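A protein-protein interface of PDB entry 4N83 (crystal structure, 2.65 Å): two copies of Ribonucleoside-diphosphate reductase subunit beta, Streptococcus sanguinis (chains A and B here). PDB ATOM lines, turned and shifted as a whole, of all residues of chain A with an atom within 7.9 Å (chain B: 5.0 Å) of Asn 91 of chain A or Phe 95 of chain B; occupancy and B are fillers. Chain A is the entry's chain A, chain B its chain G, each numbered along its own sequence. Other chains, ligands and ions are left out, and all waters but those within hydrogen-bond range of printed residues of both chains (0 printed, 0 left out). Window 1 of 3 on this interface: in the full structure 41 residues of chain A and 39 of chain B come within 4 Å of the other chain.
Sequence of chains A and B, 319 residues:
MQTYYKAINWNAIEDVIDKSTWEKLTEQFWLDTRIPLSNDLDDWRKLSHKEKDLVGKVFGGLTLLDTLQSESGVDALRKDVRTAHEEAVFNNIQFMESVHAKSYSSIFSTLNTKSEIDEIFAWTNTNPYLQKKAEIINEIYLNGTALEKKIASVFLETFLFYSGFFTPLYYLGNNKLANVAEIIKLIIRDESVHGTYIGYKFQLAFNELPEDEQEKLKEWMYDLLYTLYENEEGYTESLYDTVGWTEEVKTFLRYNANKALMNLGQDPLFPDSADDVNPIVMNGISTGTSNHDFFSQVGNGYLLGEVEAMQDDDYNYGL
Asn 91 of chain A touches Gln 94 of chain B, and with the chains exchanged Gln 94 of chain A touches Asn 91 of chain B.
Asn 91 of chain A touches Phe 95 of chain B, and with the chains exchanged Phe 95 of chain A touches Asn 91 of chain B.
Asn 92 of chain A touches Phe 95 of chain B, and with the chains exchanged Phe 95 of chain A touches Asn 92 of chain B.
Gln 94 of chain B touches its own counterpart, Gln 94 of chain A.
8 positions are printed for both chains.
Of the 16 pairs that touch across the chains among the printed residues, 9 have their exchanged pair printed and touching as well.
The backbone carbonyl oxygen (O) of Trp 22 of chain A is in hydrogen-bond range of the side-chain hydroxyl (OG1) of Thr 26 of chain A (2.6 Å).
The guanidinium group of Arg 78 of chain A sits at hydrogen-bond distance from the side-chain amide oxygen of Asn 91 of chain A (3.2 Å).
The guanidinium group (NH2) of Arg 78 of chain A lies within hydrogen-bond range of the side-chain amide oxygen (OE1) of Gln 94 of chain A, 2.7 Å away.
The backbone carbonyl oxygen (O) of Ser 70 of chain B lies within hydrogen-bond range of the side-chain amide nitrogen (NE2) of Gln 94 of chain B (2.9 Å).
O of Glu 87 of chain A lies close to ND2 of Asn 91 of chain A (3.2 Å).
O of Gln 94 of chain B lies within hydrogen-bond range of OG of Ser 98 of chain B (3.3 Å).
Among the printed residues, merely in contact across the chains: Phe 29 of chain A with Phe 29 of chain B, Asn 92 of chain A with Phe 95 of chain B, Phe 95 of chain A with Asn 92 of chain B, Gln 94 of chain A with Gln 94 of chain B, Trp 22 of chain A with Phe 95 of chain B, Phe 95 of chain A with Asn 91 of chain B, Asn 91 of chain A with Phe 95 of chain B, Phe 95 of chain A with Phe 95 of chain B, Arg 78 of chain A with Gln 94 of chain B, Ala 88 of chain A with Ser 98 of chain B and Trp 22 of chain A with Ser 98 of chain B.
The side-chain amide oxygen (OD1) of Asn 91 of chain A sits close to the side-chain amide oxygen (OE1) of Gln 94 of chain B (3.2 Å).
The side-chain amide nitrogen (ND2) of Asn 91 of chain A sits at hydrogen-bond distance from the backbone carbonyl oxygen (O) of Ser 70 of chain B, at 3.3 Å.
The side-chain carboxylate (OE2) of Glu 87 of chain A sits close to the backbone carbonyl oxygen (O) of Glu 71 of chain B (3.3 Å).
The side-chain amide nitrogen of Asn 91 of chain A sits at hydrogen-bond distance from the side-chain hydroxyl of Ser 98 of chain B, 2.8 Å away.
The side-chain amide oxygen of Gln 94 of chain A sits close to the side-chain amide oxygen of Asn 91 of chain B, at 3.4 Å.
Asn 91 of chain A touches just these residues of chain B: Ser 70, Gln 94, Phe 95 and Ser 98.
Phe 95 of chain B touches just these residues of chain A: Trp 22 (3.6 Å), Asn 91 (3.6 Å), Asn 92 (3.4 Å) and Phe 95 (3.7 Å).
Gln 94 of chain B touches three residues of chain A.
Of the printed residues of chain A, Phe 29 of chain B touches Phe 29.
Printed residues of chain A within 4 Å of Ser 98 of chain B: Trp 22, Ala 88 and Asn 91.
Of the printed residues of chain B, Phe 29 of chain A touches Phe 29 (3.3 Å).
Ala 84 of chain A touches none of the printed residues of chain B.
Of the 12 printed residues of chain B, 8 touch a printed residue of chain A.
Printed residues of chain B that touch a printed residue of chain A: Phe 29, Ser 70, Glu 71, Asn 91, Asn 92, Gln 94, Phe 95 and Ser 98.
Hydrophobic or aromatic side chains of chain B within 4 Å of the printed part of chain A: Phe 29 and Phe 95.
Printed residues of chain A that touch a printed residue of chain B: Trp 22, Phe 29, Arg 78, Glu 87, Ala 88, Asn 91, Asn 92, Gln 94 and Phe 95.
Among the printed residues, 16 pairs touch across the chains.
Among the printed residues, no Asp or Glu carboxylate lies within 4 Å of a Lys or Arg side-chain nitrogen of the other chain.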
ATOM      1  N   TRP A  22       0.858   7.505  17.517  1.00  0.00           N
ATOM      2  CA  TRP A  22       0.049   7.860  18.679  1.00  0.00           C
ATOM      3  C   TRP A  22       0.385   9.278  19.141  1.00  0.00           C
ATOM      4  O   TRP A  22      -0.510  10.102  19.328  1.00  0.00           O
ATOM      5  CB  TRP A  22       0.277   6.861  19.817  1.00  0.00           C
ATOM      6  CG  TRP A  22      -0.410   7.231  21.098  1.00  0.00           C
ATOM      7  CD1 TRP A  22       0.095   8.004  22.101  1.00  0.00           C
ATOM      8  CD2 TRP A  22      -1.722   6.838  21.517  1.00  0.00           C
ATOM      9  NE1 TRP A  22      -0.821   8.120  23.118  1.00  0.00           N
ATOM     10  CE2 TRP A  22      -1.944   7.413  22.785  1.00  0.00           C
ATOM     11  CE3 TRP A  22      -2.733   6.057  20.944  1.00  0.00           C
ATOM     12  CZ2 TRP A  22      -3.135   7.233  23.490  1.00  0.00           C
ATOM     13  CZ3 TRP A  22      -3.918   5.880  21.648  1.00  0.00           C
ATOM     14  CH2 TRP A  22      -4.105   6.464  22.907  1.00  0.00           C
ATOM     15  N   LEU A  25      -0.837  12.042  16.510  1.00  0.00           N
ATOM     16  CA  LEU A  25      -2.293  12.177  16.440  1.00  0.00           C
ATOM     17  C   LEU A  25      -2.889  12.761  17.720  1.00  0.00           C
ATOM     18  O   LEU A  25      -3.776  13.613  17.657  1.00  0.00           O
ATOM     19  CB  LEU A  25      -2.951  10.833  16.117  1.00  0.00           C
ATOM     20  CG  LEU A  25      -2.806  10.340  14.673  1.00  0.00           C
ATOM     21  CD1 LEU A  25      -3.147   8.860  14.569  1.00  0.00           C
ATOM     22  CD2 LEU A  25      -3.676  11.157  13.728  1.00  0.00           C
ATOM     23  N   THR A  26      -2.403  12.309  18.872  1.00  0.00           N
ATOM     24  CA  THR A  26      -2.854  12.848  20.155  1.00  0.00           C
ATOM     25  C   THR A  26      -2.458  14.319  20.314  1.00  0.00           C
ATOM     26  O   THR A  26      -3.227  15.122  20.841  1.00  0.00           O
ATOM     27  CB  THR A  26      -2.291  12.042  21.340  1.00  0.00           C
ATOM     28  OG1 THR A  26      -0.869  11.911  21.206  1.00  0.00           O
ATOM     29  CG2 THR A  26      -2.936  10.662  21.399  1.00  0.00           C
ATOM     30  N   GLU A  27      -1.254  14.661  19.861  1.00  0.00           N
ATOM     31  CA  GLU A  27      -0.818  16.056  19.806  1.00  0.00           C
ATOM     32  C   GLU A  27      -1.645  16.858  18.796  1.00  0.00           C
ATOM     33  O   GLU A  27      -1.818  18.068  18.953  1.00  0.00           O
ATOM     34  CB  GLU A  27       0.670  16.148  19.451  1.00  0.00           C
ATOM     35  CG  GLU A  27       1.611  15.769  20.587  1.00  0.00           C
ATOM     36  CD  GLU A  27       3.075  15.786  20.175  1.00  0.00           C
ATOM     37  OE1 GLU A  27       3.373  15.608  18.973  1.00  0.00           O
ATOM     38  OE2 GLU A  27       3.936  15.976  21.059  1.00  0.00           O
ATOM     39  N   PHE A  29      -4.830  16.715  18.451  1.00  0.00           N
ATOM     40  CA  PHE A  29      -6.214  16.704  18.941  1.00  0.00           C
ATOM     41  C   PHE A  29      -6.842  18.088  18.760  1.00  0.00           C
ATOM     42  O   PHE A  29      -6.172  19.105  18.950  1.00  0.00           O
ATOM     43  CB  PHE A  29      -6.238  16.291  20.422  1.00  0.00           C
ATOM     44  CG  PHE A  29      -7.572  16.472  21.100  1.00  0.00           C
ATOM     45  CD1 PHE A  29      -8.433  15.395  21.271  1.00  0.00           C
ATOM     46  CD2 PHE A  29      -7.952  17.714  21.598  1.00  0.00           C
ATOM     47  CE1 PHE A  29      -9.655  15.560  21.908  1.00  0.00           C
ATOM     48  CE2 PHE A  29      -9.173  17.884  22.231  1.00  0.00           C
ATOM     49  CZ  PHE A  29     -10.025  16.804  22.388  1.00  0.00           C
ATOM     50  N   VAL A  74     -13.300   2.244  10.623  1.00  0.00           N
ATOM     51  CA  VAL A  74     -12.177   1.940  11.514  1.00  0.00           C
ATOM     52  C   VAL A  74     -12.463   0.671  12.322  1.00  0.00           C
ATOM     53  O   VAL A  74     -11.536  -0.033  12.729  1.00  0.00           O
ATOM     54  CB  VAL A  74     -11.864   3.113  12.470  1.00  0.00           C
ATOM     55  CG1 VAL A  74     -10.646   2.794  13.330  1.00  0.00           C
ATOM     56  CG2 VAL A  74     -11.633   4.401  11.686  1.00  0.00           C
ATOM     57  N   ARG A  78      -9.786  -2.331  12.701  1.00  0.00           N
ATOM     58  CA  ARG A  78      -9.324  -2.729  14.037  1.00  0.00           C
ATOM     59  C   ARG A  78      -9.132  -4.239  14.190  1.00  0.00           C
ATOM     60  O   ARG A  78      -8.168  -4.680  14.818  1.00  0.00           O
ATOM     61  CB  ARG A  78     -10.293  -2.217  15.116  1.00  0.00           C
ATOM     62  CG  ARG A  78     -10.151  -2.891  16.479  1.00  0.00           C
ATOM     63  CD  ARG A  78     -10.773  -2.083  17.610  1.00  0.00           C
ATOM     64  NE  ARG A  78     -12.029  -1.446  17.216  1.00  0.00           N
ATOM     65  CZ  ARG A  78     -12.167  -0.171  16.847  1.00  0.00           C
ATOM     66  NH1 ARG A  78     -11.129   0.663  16.811  1.00  0.00           N
ATOM     67  NH2 ARG A  78     -13.369   0.276  16.508  1.00  0.00           N
ATOM     68  N   ALA A  84      -0.705  -4.577  19.801  1.00  0.00           N
ATOM     69  CA  ALA A  84      -1.720  -4.064  20.728  1.00  0.00           C
ATOM     70  C   ALA A  84      -1.852  -2.544  20.634  1.00  0.00           C
ATOM     71  O   ALA A  84      -2.945  -1.995  20.773  1.00  0.00           O
ATOM     72  CB  ALA A  84      -1.388  -4.472  22.156  1.00  0.00           C
ATOM     73  N   HIS A  85      -0.726  -1.882  20.378  1.00  0.00           N
ATOM     74  CA  HIS A  85      -0.659  -0.421  20.317  1.00  0.00           C
ATOM     75  C   HIS A  85      -1.388   0.110  19.088  1.00  0.00           C
ATOM     76  O   HIS A  85      -1.972   1.191  19.127  1.00  0.00           O
ATOM     77  CB  HIS A  85       0.801   0.046  20.299  1.00  0.00           C
ATOM     78  CG  HIS A  85       1.690  -0.724  21.226  1.00  0.00           C
ATOM     79  ND1 HIS A  85       2.509  -1.743  20.791  1.00  0.00           N
ATOM     80  CD2 HIS A  85       1.873  -0.640  22.565  1.00  0.00           C
ATOM     81  CE1 HIS A  85       3.166  -2.247  21.820  1.00  0.00           C
ATOM     82  NE2 HIS A  85       2.797  -1.595  22.908  1.00  0.00           N
ATOM     83  N   GLU A  86      -1.348  -0.660  18.004  1.00  0.00           N
ATOM     84  CA  GLU A  86      -2.066  -0.325  16.773  1.00  0.00           C
ATOM     85  C   GLU A  86      -3.572  -0.203  17.007  1.00  0.00           C
ATOM     86  O   GLU A  86      -4.218   0.677  16.442  1.00  0.00           O
ATOM     87  CB  GLU A  86      -1.783  -1.379  15.697  1.00  0.00           C
ATOM     88  CG  GLU A  86      -2.439  -1.110  14.352  1.00  0.00           C
ATOM     89  CD  GLU A  86      -2.003  -2.084  13.271  1.00  0.00           C
ATOM     90  OE1 GLU A  86      -1.196  -2.993  13.564  1.00  0.00           O
ATOM     91  OE2 GLU A  86      -2.468  -1.939  12.121  1.00  0.00           O
ATOM     92  N   GLU A  87      -4.125  -1.084  17.837  1.00  0.00           N
ATOM     93  CA  GLU A  87      -5.545  -1.025  18.176  1.00  0.00           C
ATOM     94  C   GLU A  87      -5.862   0.260  18.938  1.00  0.00           C
ATOM     95  O   GLU A  87      -6.889   0.892  18.695  1.00  0.00           O
ATOM     96  CB  GLU A  87      -5.973  -2.254  18.989  1.00  0.00           C
ATOM     97  CG  GLU A  87      -7.484  -2.377  19.160  1.00  0.00           C
ATOM     98  CD  GLU A  87      -7.959  -3.794  19.456  1.00  0.00           C
ATOM     99  OE1 GLU A  87      -7.129  -4.729  19.472  1.00  0.00           O
ATOM    100  OE2 GLU A  87      -9.177  -3.974  19.670  1.00  0.00           O
ATOM    101  N   ALA A  88      -4.969   0.645  19.849  1.00  0.00           N
ATOM    102  CA  ALA A  88      -5.096   1.914  20.571  1.00  0.00           C
ATOM    103  C   ALA A  88      -5.063   3.100  19.603  1.00  0.00           C
ATOM    104  O   ALA A  88      -5.893   4.005  19.696  1.00  0.00           O
ATOM    105  CB  ALA A  88      -3.998   2.049  21.617  1.00  0.00           C
ATOM    106  N   VAL A  89      -4.114   3.081  18.670  1.00  0.00           N
ATOM    107  CA  VAL A  89      -4.026   4.124  17.645  1.00  0.00           C
ATOM    108  C   VAL A  89      -5.341   4.211  16.865  1.00  0.00           C
ATOM    109  O   VAL A  89      -5.821   5.306  16.584  1.00  0.00           O
ATOM    110  CB  VAL A  89      -2.851   3.888  16.667  1.00  0.00           C
ATOM    111  CG1 VAL A  89      -2.848   4.936  15.562  1.00  0.00           C
ATOM    112  CG2 VAL A  89      -1.521   3.910  17.409  1.00  0.00           C
ATOM    113  N   PHE A  90      -5.925   3.059  16.536  1.00  0.00           N
ATOM    114  CA  PHE A  90      -7.198   3.016  15.804  1.00  0.00           C
ATOM    115  C   PHE A  90      -8.386   3.518  16.623  1.00  0.00           C
ATOM    116  O   PHE A  90      -9.355   4.025  16.057  1.00  0.00           O
ATOM    117  CB  PHE A  90      -7.480   1.610  15.256  1.00  0.00           C
ATOM    118  CG  PHE A  90      -6.782   1.320  13.957  1.00  0.00           C
ATOM    119  CD1 PHE A  90      -7.056   2.083  12.831  1.00  0.00           C
ATOM    120  CD2 PHE A  90      -5.857   0.292  13.855  1.00  0.00           C
ATOM    121  CE1 PHE A  90      -6.416   1.831  11.631  1.00  0.00           C
ATOM    122  CE2 PHE A  90      -5.214   0.034  12.656  1.00  0.00           C
ATOM    123  CZ  PHE A  90      -5.494   0.804  11.543  1.00  0.00           C
ATOM    124  N   ASN A  91      -8.315   3.379  17.945  1.00  0.00           N
ATOM    125  CA  ASN A  91      -9.329   3.968  18.823  1.00  0.00           C
ATOM    126  C   ASN A  91      -9.271   5.486  18.743  1.00  0.00           C
ATOM    127  O   ASN A  91     -10.305   6.150  18.645  1.00  0.00           O
ATOM    128  CB  ASN A  91      -9.141   3.512  20.273  1.00  0.00           C
ATOM    129  CG  ASN A  91      -9.348   2.019  20.448  1.00  0.00           C
ATOM    130  OD1 ASN A  91     -10.164   1.407  19.755  1.00  0.00           O
ATOM    131  ND2 ASN A  91      -8.611   1.426  21.384  1.00  0.00           N
ATOM    132  N   ASN A  92      -8.050   6.021  18.776  1.00  0.00           N
ATOM    133  CA  ASN A  92      -7.813   7.445  18.550  1.00  0.00           C
ATOM    134  C   ASN A  92      -8.245   7.882  17.149  1.00  0.00           C
ATOM    135  O   ASN A  92      -8.859   8.936  16.989  1.00  0.00           O
ATOM    136  CB  ASN A  92      -6.333   7.784  18.762  1.00  0.00           C
ATOM    137  CG  ASN A  92      -5.981   9.176  18.282  1.00  0.00           C
ATOM    138  OD1 ASN A  92      -5.392   9.338  17.216  1.00  0.00           O
ATOM    139  ND2 ASN A  92      -6.365  10.189  19.050  1.00  0.00           N
ATOM    140  N   ILE A  93      -7.916   7.073  16.143  1.00  0.00           N
ATOM    141  CA  ILE A  93      -8.310   7.361  14.763  1.00  0.00           C
ATOM    142  C   ILE A  93      -9.829   7.430  14.650  1.00  0.00           C
ATOM    143  O   ILE A  93     -10.367   8.386  14.095  1.00  0.00           O
ATOM    144  CB  ILE A  93      -7.770   6.305  13.769  1.00  0.00           C
ATOM    145  CG1 ILE A  93      -6.244   6.402  13.665  1.00  0.00           C
ATOM    146  CG2 ILE A  93      -8.396   6.495  12.390  1.00  0.00           C
ATOM    147  CD1 ILE A  93      -5.574   5.189  13.054  1.00  0.00           C
ATOM    148  N   GLN A  94     -10.510   6.422  15.190  1.00  0.00           N
ATOM    149  CA  GLN A  94     -11.968   6.330  15.091  1.00  0.00           C
ATOM    150  C   GLN A  94     -12.685   7.492  15.774  1.00  0.00           C
ATOM    151  O   GLN A  94     -13.703   7.976  15.270  1.00  0.00           O
ATOM    152  CB  GLN A  94     -12.469   5.013  15.681  1.00  0.00           C
ATOM    153  CG  GLN A  94     -13.925   4.732  15.354  1.00  0.00           C
ATOM    154  CD  GLN A  94     -14.382   3.372  15.832  1.00  0.00           C
ATOM    155  OE1 GLN A  94     -13.932   2.884  16.869  1.00  0.00           O
ATOM    156  NE2 GLN A  94     -15.284   2.748  15.076  1.00  0.00           N
ATOM    157  N   PHE A  95     -12.165   7.922  16.922  1.00  0.00           N
ATOM    158  CA  PHE A  95     -12.714   9.081  17.628  1.00  0.00           C
ATOM    159  C   PHE A  95     -12.580  10.356  16.794  1.00  0.00           C
ATOM    160  O   PHE A  95     -13.535  11.123  16.672  1.00  0.00           O
ATOM    161  CB  PHE A  95     -12.041   9.266  18.992  1.00  0.00           C
ATOM    162  CG  PHE A  95     -12.194  10.649  19.563  1.00  0.00           C
ATOM    163  CD1 PHE A  95     -13.455  11.183  19.802  1.00  0.00           C
ATOM    164  CD2 PHE A  95     -11.078  11.418  19.860  1.00  0.00           C
ATOM    165  CE1 PHE A  95     -13.596  12.460  20.319  1.00  0.00           C
ATOM    166  CE2 PHE A  95     -11.213  12.692  20.382  1.00  0.00           C
ATOM    167  CZ  PHE A  95     -12.473  13.215  20.613  1.00  0.00           C
ATOM    168  N   MET A  96     -11.400  10.577  16.219  1.00  0.00           N
ATOM    169  CA  MET A  96     -11.166  11.757  15.383  1.00  0.00           C
ATOM    170  C   MET A  96     -12.022  11.749  14.114  1.00  0.00           C
ATOM    171  O   MET A  96     -12.377  12.811  13.607  1.00  0.00           O
ATOM    172  CB  MET A  96      -9.679  11.894  15.023  1.00  0.00           C
ATOM    173  CG  MET A  96      -8.767  12.243  16.194  1.00  0.00           C
ATOM    174  SD  MET A  96      -9.330  13.628  17.208  1.00  0.00           S
ATOM    175  CE  MET A  96      -9.570  14.898  15.968  1.00  0.00           C
ATOM    176  N   GLU A  97     -12.357  10.562  13.610  1.00  0.00           N
ATOM    177  CA  GLU A  97     -13.261  10.448  12.462  1.00  0.00           C
ATOM    178  C   GLU A  97     -14.672  10.932  12.820  1.00  0.00           C
ATOM    179  O   GLU A  97     -15.375  11.477  11.969  1.00  0.00           O
ATOM    180  CB  GLU A  97     -13.317   9.007  11.932  1.00  0.00           C
ATOM    181  CG  GLU A  97     -11.994   8.449  11.410  1.00  0.00           C
ATOM    182  CD  GLU A  97     -11.529   9.069  10.102  1.00  0.00           C
ATOM    183  OE1 GLU A  97     -12.146  10.048   9.632  1.00  0.00           O
ATOM    184  OE2 GLU A  97     -10.529   8.574   9.539  1.00  0.00           O
ATOM    185  N   PHE B  29     -10.811  16.077  27.770  1.00  0.00           N
ATOM    186  CA  PHE B  29      -9.663  15.426  27.138  1.00  0.00           C
ATOM    187  C   PHE B  29      -8.374  15.758  27.876  1.00  0.00           C
ATOM    188  O   PHE B  29      -8.147  16.910  28.248  1.00  0.00           O
ATOM    189  CB  PHE B  29      -9.528  15.839  25.670  1.00  0.00           C
ATOM    190  CG  PHE B  29      -8.236  15.398  25.036  1.00  0.00           C
ATOM    191  CD1 PHE B  29      -7.940  14.047  24.909  1.00  0.00           C
ATOM    192  CD2 PHE B  29      -7.313  16.328  24.576  1.00  0.00           C
ATOM    193  CE1 PHE B  29      -6.753  13.631  24.333  1.00  0.00           C
ATOM    194  CE2 PHE B  29      -6.123  15.918  23.998  1.00  0.00           C
ATOM    195  CZ  PHE B  29      -5.844  14.568  23.874  1.00  0.00           C
ATOM    196  N   SER B  70     -10.738  -0.906  26.268  1.00  0.00           N
ATOM    197  CA  SER B  70     -10.338  -0.245  25.024  1.00  0.00           C
ATOM    198  C   SER B  70     -10.376  -1.188  23.815  1.00  0.00           C
ATOM    199  O   SER B  70     -10.681  -0.756  22.702  1.00  0.00           O
ATOM    200  CB  SER B  70      -8.942   0.376  25.164  1.00  0.00           C
ATOM    201  OG  SER B  70      -8.006  -0.551  25.685  1.00  0.00           O
ATOM    202  N   GLU B  71     -10.074  -2.468  24.038  1.00  0.00           N
ATOM    203  CA  GLU B  71     -10.006  -3.453  22.952  1.00  0.00           C
ATOM    204  C   GLU B  71     -11.363  -4.086  22.630  1.00  0.00           C
ATOM    205  O   GLU B  71     -11.900  -3.880  21.541  1.00  0.00           O
ATOM    206  CB  GLU B  71      -8.982  -4.547  23.279  1.00  0.00           C
ATOM    207  CG  GLU B  71      -7.539  -4.059  23.268  1.00  0.00           C
ATOM    208  CD  GLU B  71      -6.522  -5.166  23.491  1.00  0.00           C
ATOM    209  OE1 GLU B  71      -6.896  -6.359  23.450  1.00  0.00           O
ATOM    210  OE2 GLU B  71      -5.336  -4.840  23.703  1.00  0.00           O
ATOM    211  N   ASN B  91     -17.052   6.111  20.719  1.00  0.00           N
ATOM    212  CA  ASN B  91     -15.735   6.197  20.077  1.00  0.00           C
ATOM    213  C   ASN B  91     -14.759   7.059  20.885  1.00  0.00           C
ATOM    214  O   ASN B  91     -13.580   6.711  21.014  1.00  0.00           O
ATOM    215  CB  ASN B  91     -15.855   6.733  18.646  1.00  0.00           C
ATOM    216  CG  ASN B  91     -16.633   5.802  17.733  1.00  0.00           C
ATOM    217  OD1 ASN B  91     -16.634   4.583  17.918  1.00  0.00           O
ATOM    218  ND2 ASN B  91     -17.306   6.375  16.740  1.00  0.00           N
ATOM    219  N   ASN B  92     -15.251   8.181  21.415  1.00  0.00           N
ATOM    220  CA  ASN B  92     -14.484   9.001  22.359  1.00  0.00           C
ATOM    221  C   ASN B  92     -14.133   8.187  23.594  1.00  0.00           C
ATOM    222  O   ASN B  92     -12.976   8.137  24.005  1.00  0.00           O
ATOM    223  CB  ASN B  92     -15.271  10.258  22.765  1.00  0.00           C
ATOM    224  CG  ASN B  92     -14.705  10.935  24.008  1.00  0.00           C
ATOM    225  OD1 ASN B  92     -14.898  10.461  25.127  1.00  0.00           O
ATOM    226  ND2 ASN B  92     -14.014  12.054  23.819  1.00  0.00           N
ATOM    227  N   ILE B  93     -15.150   7.557  24.177  1.00  0.00           N
ATOM    228  CA  ILE B  93     -14.981   6.719  25.362  1.00  0.00           C
ATOM    229  C   ILE B  93     -13.898   5.664  25.139  1.00  0.00           C
ATOM    230  O   ILE B  93     -13.015   5.507  25.975  1.00  0.00           O
ATOM    231  CB  ILE B  93     -16.315   6.044  25.778  1.00  0.00           C
ATOM    232  CG1 ILE B  93     -17.254   7.080  26.408  1.00  0.00           C
ATOM    233  CG2 ILE B  93     -16.075   4.904  26.761  1.00  0.00           C
ATOM    234  CD1 ILE B  93     -18.706   6.650  26.484  1.00  0.00           C
ATOM    235  N   GLN B  94     -13.957   4.963  24.007  1.00  0.00           N
ATOM    236  CA  GLN B  94     -13.003   3.885  23.725  1.00  0.00           C
ATOM    237  C   GLN B  94     -11.571   4.395  23.560  1.00  0.00           C
ATOM    238  O   GLN B  94     -10.621   3.702  23.933  1.00  0.00           O
ATOM    239  CB  GLN B  94     -13.411   3.089  22.482  1.00  0.00           C
ATOM    240  CG  GLN B  94     -12.677   1.761  22.364  1.00  0.00           C
ATOM    241  CD  GLN B  94     -13.071   0.968  21.135  1.00  0.00           C
ATOM    242  OE1 GLN B  94     -13.305   1.535  20.067  1.00  0.00           O
ATOM    243  NE2 GLN B  94     -13.128  -0.355  21.273  1.00  0.00           N
ATOM    244  N   PHE B  95     -11.419   5.590  22.991  1.00  0.00           N
ATOM    245  CA  PHE B  95     -10.102   6.221  22.866  1.00  0.00           C
ATOM    246  C   PHE B  95      -9.529   6.533  24.245  1.00  0.00           C
ATOM    247  O   PHE B  95      -8.376   6.213  24.524  1.00  0.00           O
ATOM    248  CB  PHE B  95     -10.177   7.493  22.010  1.00  0.00           C
ATOM    249  CG  PHE B  95      -9.011   8.429  22.201  1.00  0.00           C
ATOM    250  CD1 PHE B  95      -7.711   8.005  21.958  1.00  0.00           C
ATOM    251  CD2 PHE B  95      -9.215   9.738  22.621  1.00  0.00           C
ATOM    252  CE1 PHE B  95      -6.638   8.865  22.137  1.00  0.00           C
ATOM    253  CE2 PHE B  95      -8.145  10.603  22.797  1.00  0.00           C
ATOM    254  CZ  PHE B  95      -6.855  10.166  22.553  1.00  0.00           C
ATOM    255  N   MET B  96     -10.344   7.144  25.103  1.00  0.00           N
ATOM    256  CA  MET B  96      -9.908   7.518  26.450  1.00  0.00           C
ATOM    257  C   MET B  96      -9.578   6.301  27.326  1.00  0.00           C
ATOM    258  O   MET B  96      -8.807   6.423  28.275  1.00  0.00           O
ATOM    259  CB  MET B  96     -10.963   8.394  27.144  1.00  0.00           C
ATOM    260  CG  MET B  96     -11.225   9.738  26.473  1.00  0.00           C
ATOM    261  SD  MET B  96      -9.776  10.804  26.299  1.00  0.00           S
ATOM    262  CE  MET B  96      -9.423  11.207  28.008  1.00  0.00           C
ATOM    263  N   GLU B  97     -10.150   5.138  27.012  1.00  0.00           N
ATOM    264  CA  GLU B  97      -9.788   3.895  27.702  1.00  0.00           C
ATOM    265  C   GLU B  97      -8.361   3.478  27.338  1.00  0.00           C
ATOM    266  O   GLU B  97      -7.638   2.935  28.172  1.00  0.00           O
ATOM    267  CB  GLU B  97     -10.765   2.755  27.372  1.00  0.00           C
ATOM    268  CG  GLU B  97     -12.210   2.984  27.805  1.00  0.00           C
ATOM    269  CD  GLU B  97     -12.414   2.998  29.311  1.00  0.00           C
ATOM    270  OE1 GLU B  97     -11.444   2.773  30.065  1.00  0.00           O
ATOM    271  OE2 GLU B  97     -13.562   3.239  29.745  1.00  0.00           O
ATOM    272  N   SER B  98      -7.967   3.731  26.090  1.00  0.00           N
ATOM    273  CA  SER B  98      -6.593   3.490  25.650  1.00  0.00           C
ATOM    274  C   SER B  98      -5.633   4.483  26.304  1.00  0.00           C
ATOM    275  O   SER B  98      -4.481   4.143  26.589  1.00  0.00           O
ATOM    276  CB  SER B  98      -6.482   3.588  24.126  1.00  0.00           C
ATOM    277  OG  SER B  98      -7.474   2.809  23.482  1.00  0.00           O
ATOM    278  N   VAL B  99      -6.110   5.710  26.529  1.00  0.00           N
ATOM    279  CA  VAL B  99      -5.339   6.737  27.236  1.00  0.00           C
ATOM    280  C   VAL B  99      -5.107   6.301  28.677  1.00  0.00           C
ATOM    281  O   VAL B  99      -4.014   6.482  29.217  1.00  0.00           O
ATOM    282  CB  VAL B  99      -6.052   8.112  27.237  1.00  0.00           C
ATOM    283  CG1 VAL B  99      -5.277   9.127  28.075  1.00  0.00           C
ATOM    284  CG2 VAL B  99      -6.233   8.629  25.817  1.00  0.00           C
